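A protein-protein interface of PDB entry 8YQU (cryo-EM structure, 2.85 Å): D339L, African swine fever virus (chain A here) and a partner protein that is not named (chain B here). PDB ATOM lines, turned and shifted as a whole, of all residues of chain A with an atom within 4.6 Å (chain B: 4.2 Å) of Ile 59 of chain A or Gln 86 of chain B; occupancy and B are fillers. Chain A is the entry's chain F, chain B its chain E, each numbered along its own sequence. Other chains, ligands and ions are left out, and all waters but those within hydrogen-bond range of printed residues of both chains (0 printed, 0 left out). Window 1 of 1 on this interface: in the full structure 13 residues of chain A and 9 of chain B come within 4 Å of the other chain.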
ATOM      1  N   PRO A  16      12.166   1.781   9.487  1.00  0.00           N
ATOM      2  CA  PRO A  16      11.482   1.214   8.314  1.00  0.00           C
ATOM      3  C   PRO A  16      11.136   2.237   7.245  1.00  0.00           C
ATOM      4  O   PRO A  16      11.152   1.898   6.054  1.00  0.00           O
ATOM      5  CB  PRO A  16      10.220   0.587   8.922  1.00  0.00           C
ATOM      6  CG  PRO A  16      10.547   0.387  10.368  1.00  0.00           C
ATOM      7  CD  PRO A  16      11.417   1.543  10.731  1.00  0.00           C
ATOM      8  N   THR A  17      10.824   3.476   7.628  1.00  0.00           N
ATOM      9  CA  THR A  17      10.384   4.469   6.652  1.00  0.00           C
ATOM     10  C   THR A  17      11.489   4.792   5.653  1.00  0.00           C
ATOM     11  O   THR A  17      11.265   4.778   4.437  1.00  0.00           O
ATOM     12  CB  THR A  17       9.917   5.737   7.367  1.00  0.00           C
ATOM     13  OG1 THR A  17       9.064   5.383   8.463  1.00  0.00           O
ATOM     14  CG2 THR A  17       9.153   6.636   6.409  1.00  0.00           C
ATOM     15  N   CYS A  57       8.311  -5.949   4.894  1.00  0.00           N
ATOM     16  CA  CYS A  57       8.944  -5.384   6.077  1.00  0.00           C
ATOM     17  C   CYS A  57       7.967  -5.384   7.245  1.00  0.00           C
ATOM     18  O   CYS A  57       7.178  -4.446   7.403  1.00  0.00           O
ATOM     19  CB  CYS A  57       9.447  -3.967   5.800  1.00  0.00           C
ATOM     20  SG  CYS A  57      10.250  -3.176   7.213  1.00  0.00           S
ATOM     21  N   PHE A  58       8.008  -6.432   8.062  1.00  0.00           N
ATOM     22  CA  PHE A  58       7.123  -6.516   9.210  1.00  0.00           C
ATOM     23  C   PHE A  58       7.565  -5.537  10.294  1.00  0.00           C
ATOM     24  O   PHE A  58       8.685  -5.021  10.293  1.00  0.00           O
ATOM     25  CB  PHE A  58       7.100  -7.934   9.778  1.00  0.00           C
ATOM     26  CG  PHE A  58       6.720  -8.989   8.782  1.00  0.00           C
ATOM     27  CD1 PHE A  58       5.393  -9.211   8.461  1.00  0.00           C
ATOM     28  CD2 PHE A  58       7.687  -9.778   8.186  1.00  0.00           C
ATOM     29  CE1 PHE A  58       5.040 -10.186   7.550  1.00  0.00           C
ATOM     30  CE2 PHE A  58       7.341 -10.754   7.276  1.00  0.00           C
ATOM     31  CZ  PHE A  58       6.015 -10.958   6.958  1.00  0.00           C
ATOM     32  N   ILE A  59       6.658  -5.284  11.233  1.00  0.00           N
ATOM     33  CA  ILE A  59       6.942  -4.496  12.426  1.00  0.00           C
ATOM     34  C   ILE A  59       7.026  -5.455  13.603  1.00  0.00           C
ATOM     35  O   ILE A  59       6.130  -6.286  13.797  1.00  0.00           O
ATOM     36  CB  ILE A  59       5.869  -3.419  12.664  1.00  0.00           C
ATOM     37  CG1 ILE A  59       5.756  -2.501  11.446  1.00  0.00           C
ATOM     38  CG2 ILE A  59       6.193  -2.612  13.908  1.00  0.00           C
ATOM     39  CD1 ILE A  59       7.050  -1.824  11.075  1.00  0.00           C
ATOM     40  N   MET A  60       8.106  -5.354  14.375  1.00  0.00           N
ATOM     41  CA  MET A  60       8.314  -6.264  15.493  1.00  0.00           C
ATOM     42  C   MET A  60       7.162  -6.171  16.485  1.00  0.00           C
ATOM     43  O   MET A  60       6.709  -5.078  16.836  1.00  0.00           O
ATOM     44  CB  MET A  60       9.646  -5.968  16.176  1.00  0.00           C
ATOM     45  CG  MET A  60      10.748  -5.594  15.204  1.00  0.00           C
ATOM     46  SD  MET A  60      12.394  -5.994  15.809  1.00  0.00           S
ATOM     47  CE  MET A  60      12.328  -5.216  17.413  1.00  0.00           C
ATOM     48  N   ARG A  61       6.693  -7.333  16.933  1.00  0.00           N
ATOM     49  CA  ARG A  61       5.455  -7.452  17.686  1.00  0.00           C
ATOM     50  C   ARG A  61       5.660  -7.552  19.191  1.00  0.00           C
ATOM     51  O   ARG A  61       4.738  -7.231  19.947  1.00  0.00           O
ATOM     52  CB  ARG A  61       4.678  -8.682  17.193  1.00  0.00           C
ATOM     53  CG  ARG A  61       3.201  -8.711  17.532  1.00  0.00           C
ATOM     54  CD  ARG A  61       2.938  -9.596  18.739  1.00  0.00           C
ATOM     55  NE  ARG A  61       3.234 -10.996  18.458  1.00  0.00           N
ATOM     56  CZ  ARG A  61       3.377 -11.932  19.386  1.00  0.00           C
ATOM     57  NH1 ARG A  61       3.254 -11.654  20.672  1.00  0.00           N
ATOM     58  NH2 ARG A  61       3.652 -13.178  19.012  1.00  0.00           N
ATOM     59  N   GLY A  66       8.809   0.014  17.759  1.00  0.00           N
ATOM     60  CA  GLY A  66       8.409   0.408  16.424  1.00  0.00           C
ATOM     61  C   GLY A  66       9.395   0.046  15.341  1.00  0.00           C
ATOM     62  O   GLY A  66       9.242   0.497  14.203  1.00  0.00           O
ATOM     63  N   ARG A  67      10.403  -0.759  15.663  1.00  0.00           N
ATOM     64  CA  ARG A  67      11.434  -1.164  14.725  1.00  0.00           C
ATOM     65  C   ARG A  67      10.895  -2.296  13.850  1.00  0.00           C
ATOM     66  O   ARG A  67       9.842  -2.875  14.128  1.00  0.00           O
ATOM     67  CB  ARG A  67      12.704  -1.517  15.506  1.00  0.00           C
ATOM     68  CG  ARG A  67      13.932  -1.821  14.678  1.00  0.00           C
ATOM     69  CD  ARG A  67      15.190  -2.010  15.524  1.00  0.00           C
ATOM     70  NE  ARG A  67      15.158  -3.160  16.418  1.00  0.00           N
ATOM     71  CZ  ARG A  67      15.168  -3.070  17.741  1.00  0.00           C
ATOM     72  NH1 ARG A  67      15.175  -1.897  18.354  1.00  0.00           N
ATOM     73  NH2 ARG A  67      15.184  -4.183  18.468  1.00  0.00           N
ATOM     74  N   GLY A  68      11.590  -2.601  12.750  1.00  0.00           N
ATOM     75  CA  GLY A  68      11.110  -3.559  11.779  1.00  0.00           C
ATOM     76  C   GLY A  68      12.082  -4.709  11.557  1.00  0.00           C
ATOM     77  O   GLY A  68      13.221  -4.695  12.028  1.00  0.00           O
ATOM     78  N   TYR A  69      11.614  -5.708  10.810  1.00  0.00           N
ATOM     79  CA  TYR A  69      12.461  -6.831  10.434  1.00  0.00           C
ATOM     80  C   TYR A  69      11.988  -7.392   9.101  1.00  0.00           C
ATOM     81  O   TYR A  69      10.837  -7.201   8.703  1.00  0.00           O
ATOM     82  CB  TYR A  69      12.463  -7.927  11.506  1.00  0.00           C
ATOM     83  CG  TYR A  69      11.132  -8.613  11.705  1.00  0.00           C
ATOM     84  CD1 TYR A  69      10.152  -8.049  12.509  1.00  0.00           C
ATOM     85  CD2 TYR A  69      10.863  -9.835  11.104  1.00  0.00           C
ATOM     86  CE1 TYR A  69       8.939  -8.675  12.698  1.00  0.00           C
ATOM     87  CE2 TYR A  69       9.652 -10.467  11.288  1.00  0.00           C
ATOM     88  CZ  TYR A  69       8.694  -9.884  12.087  1.00  0.00           C
ATOM     89  OH  TYR A  69       7.486 -10.511  12.273  1.00  0.00           O
ATOM     90  N   ARG B  78      -3.298  -0.067  16.969  1.00  0.00           N
ATOM     91  CA  ARG B  78      -1.963  -0.549  16.633  1.00  0.00           C
ATOM     92  C   ARG B  78      -1.339   0.282  15.518  1.00  0.00           C
ATOM     93  O   ARG B  78      -0.150   0.615  15.575  1.00  0.00           O
ATOM     94  CB  ARG B  78      -2.025  -2.024  16.241  1.00  0.00           C
ATOM     95  CG  ARG B  78      -0.716  -2.597  15.730  1.00  0.00           C
ATOM     96  CD  ARG B  78       0.330  -2.716  16.823  1.00  0.00           C
ATOM     97  NE  ARG B  78       1.493  -3.461  16.358  1.00  0.00           N
ATOM     98  CZ  ARG B  78       2.659  -3.510  16.987  1.00  0.00           C
ATOM     99  NH1 ARG B  78       2.863  -2.852  18.116  1.00  0.00           N
ATOM    100  NH2 ARG B  78       3.647  -4.231  16.466  1.00  0.00           N
ATOM    101  N   VAL B  82       2.058   2.430  16.096  1.00  0.00           N
ATOM    102  CA  VAL B  82       3.238   2.156  15.282  1.00  0.00           C
ATOM    103  C   VAL B  82       3.676   3.411  14.543  1.00  0.00           C
ATOM    104  O   VAL B  82       4.869   3.743  14.503  1.00  0.00           O
ATOM    105  CB  VAL B  82       2.959   0.992  14.314  1.00  0.00           C
ATOM    106  CG1 VAL B  82       3.995   0.958  13.203  1.00  0.00           C
ATOM    107  CG2 VAL B  82       2.935  -0.328  15.064  1.00  0.00           C
ATOM    108  N   ARG B  83       2.721   4.134  13.953  1.00  0.00           N
ATOM    109  CA  ARG B  83       3.067   5.350  13.227  1.00  0.00           C
ATOM    110  C   ARG B  83       3.632   6.412  14.161  1.00  0.00           C
ATOM    111  O   ARG B  83       4.578   7.119  13.801  1.00  0.00           O
ATOM    112  CB  ARG B  83       1.845   5.879  12.478  1.00  0.00           C
ATOM    113  CG  ARG B  83       2.152   7.055  11.572  1.00  0.00           C
ATOM    114  CD  ARG B  83       3.272   6.710  10.607  1.00  0.00           C
ATOM    115  NE  ARG B  83       3.730   7.874   9.860  1.00  0.00           N
ATOM    116  CZ  ARG B  83       4.926   7.976   9.298  1.00  0.00           C
ATOM    117  NH1 ARG B  83       5.815   7.001   9.382  1.00  0.00           N
ATOM    118  NH2 ARG B  83       5.239   9.086   8.636  1.00  0.00           N
ATOM    119  N   ALA B  84       3.068   6.539  15.365  1.00  0.00           N
ATOM    120  CA  ALA B  84       3.577   7.514  16.323  1.00  0.00           C
ATOM    121  C   ALA B  84       4.997   7.177  16.754  1.00  0.00           C
ATOM    122  O   ALA B  84       5.850   8.066  16.853  1.00  0.00           O
ATOM    123  CB  ALA B  84       2.651   7.587  17.536  1.00  0.00           C
ATOM    124  N   GLN B  85       5.273   5.898  17.015  1.00  0.00           N
ATOM    125  CA  GLN B  85       6.629   5.509  17.393  1.00  0.00           C
ATOM    126  C   GLN B  85       7.612   5.749  16.253  1.00  0.00           C
ATOM    127  O   GLN B  85       8.727   6.237  16.478  1.00  0.00           O
ATOM    128  CB  GLN B  85       6.655   4.047  17.831  1.00  0.00           C
ATOM    129  CG  GLN B  85       8.017   3.582  18.304  1.00  0.00           C
ATOM    130  CD  GLN B  85       8.465   4.287  19.567  1.00  0.00           C
ATOM    131  OE1 GLN B  85       7.746   4.310  20.566  1.00  0.00           O
ATOM    132  NE2 GLN B  85       9.655   4.872  19.528  1.00  0.00           N
ATOM    133  N   GLN B  86       7.216   5.423  15.021  1.00  0.00           N
ATOM    134  CA  GLN B  86       8.102   5.654  13.884  1.00  0.00           C
ATOM    135  C   GLN B  86       8.351   7.142  13.667  1.00  0.00           C
ATOM    136  O   GLN B  86       9.462   7.543  13.303  1.00  0.00           O
ATOM    137  CB  GLN B  86       7.523   5.007  12.629  1.00  0.00           C
ATOM    138  CG  GLN B  86       7.553   3.491  12.664  1.00  0.00           C
ATOM    139  CD  GLN B  86       6.950   2.868  11.429  1.00  0.00           C
ATOM    140  OE1 GLN B  86       6.436   3.564  10.555  1.00  0.00           O
ATOM    141  NE2 GLN B  86       7.009   1.545  11.347  1.00  0.00           N
ATOM    142  N   LEU B  87       7.327   7.974  13.876  1.00  0.00           N
ATOM    143  CA  LEU B  87       7.520   9.419  13.808  1.00  0.00           C
ATOM    144  C   LEU B  87       8.464   9.897  14.902  1.00  0.00           C
ATOM    145  O   LEU B  87       9.294  10.783  14.671  1.00  0.00           O
ATOM    146  CB  LEU B  87       6.174  10.132  13.913  1.00  0.00           C
ATOM    147  CG  LEU B  87       5.296  10.099  12.664  1.00  0.00           C
ATOM    148  CD1 LEU B  87       3.869  10.456  13.021  1.00  0.00           C
ATOM    149  CD2 LEU B  87       5.837  11.045  11.609  1.00  0.00           C
ATOM    150  N   ALA B  88       8.347   9.328  16.102  1.00  0.00           N
ATOM    151  CA  ALA B  88       9.307   9.625  17.156  1.00  0.00           C
ATOM    152  C   ALA B  88      10.715   9.191  16.777  1.00  0.00           C
ATOM    153  O   ALA B  88      11.686   9.770  17.274  1.00  0.00           O
ATOM    154  CB  ALA B  88       8.884   8.952  18.462  1.00  0.00           C
ATOM    155  N   ILE B  89      10.848   8.193  15.905  1.00  0.00           N
ATOM    156  CA  ILE B  89      12.161   7.775  15.424  1.00  0.00           C
ATOM    157  C   ILE B  89      12.602   8.670  14.273  1.00  0.00           C
ATOM    158  O   ILE B  89      13.664   9.300  14.336  1.00  0.00           O
ATOM    159  CB  ILE B  89      12.159   6.296  14.994  1.00  0.00           C
ATOM    160  CG1 ILE B  89      11.892   5.388  16.193  1.00  0.00           C
ATOM    161  CG2 ILE B  89      13.482   5.935  14.340  1.00  0.00           C
ATOM    162  CD1 ILE B  89      11.676   3.937  15.819  1.00  0.00           C
ATOM    163  N   ASN B  90      11.795   8.735  13.214  1.00  0.00           N
ATOM    164  CA  ASN B  90      12.179   9.458  12.003  1.00  0.00           C
ATOM    165  C   ASN B  90      11.657  10.893  11.995  1.00  0.00           C
ATOM    166  O   ASN B  90      12.441  11.845  11.921  1.00  0.00           O
ATOM    167  CB  ASN B  90      11.682   8.703  10.765  1.00  0.00           C
ATOM    168  CG  ASN B  90      12.418   9.105   9.503  1.00  0.00           C
ATOM    169  OD1 ASN B  90      13.301   9.961   9.533  1.00  0.00           O
ATOM    170  ND2 ASN B  90      12.059   8.485   8.386  1.00  0.00           N
ATOM    171  N   GLY B  91      10.339  11.063  12.063  1.00  0.00           N
ATOM    172  CA  GLY B  91       9.734  12.377  12.011  1.00  0.00           C
ATOM    173  C   GLY B  91       9.373  12.871  10.628  1.00  0.00           C
ATOM    174  O   GLY B  91       8.794  13.958  10.509  1.00  0.00           O
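Hydrophobic or aromatic side chains of chain A within 4 Å of the printed part of chain B: Pro 16 and Ile 59. Among the printed residues, 10 pairs touch across the chains. Among the printed residues, no Asp or Glu carboxylate lies within 4 Å of a Lys or Arg side-chain nitrogen of the other chain.
Of chain B, only Arg 78 and Gln 86 come within 4 Å of Ile 59 of chain A. Of the printed residues of chain A, Arg 78 of chain B touches Ile 59, Met 60 and Arg 61. Of the printed residues of chain B, Pro 16 of chain A touches Gln 86 (3.8 Å). Of the printed residues of chain B, Met 60 of chain A touches Arg 78 (3.2 Å). Arg 67 of chain A touches none of the printed residues of chain B. Leu 87 of chain B touches none of the printed residues of chain A. The nearest printed residue of chain A that does not touch Gln 86 of chain B is Arg 67 of chain A (5.9 Å). The nearest printed residue of chain B that does not touch Met 60 of chain A is Val 82 of chain B (6.3 Å).
O of Met 60 of chain A is in hydrogen-bond range of NH2 of Arg 78 of chain B, 3.2 Å away.
NE2 of Gln 86 of chain B touches CG of Pro 16 of chain A, at 3.8 Å. Thr 17 of chain A touches Arg 83 of chain B (OG1 to NH1, 3.7 Å). OG1 of Thr 17 of chain A touches OE1 of Gln 86 of chain B, at 3.8 Å. ND2 of Asn 90 of chain B touches CB of Thr 17 of chain A (3.6 Å). CG2 of Ile 59 of chain A touches NH2 of Arg 78 of chain B, 3.96 Å away. Ile 59 of chain A touches Gln 86 of chain B. CA of Arg 61 of chain A touches NH2 of Arg 78 of chain B (3.9 Å). Gly 66 of chain A touches Gln 85 of chain B. Gly 66 of chain A touches Gln 86 of chain B.
The backbone NH of Met 60 of chain A lies within hydrogen-bond range of the backbone carbonyl oxygen of Arg 67 of chain A, 3.0 Å away.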
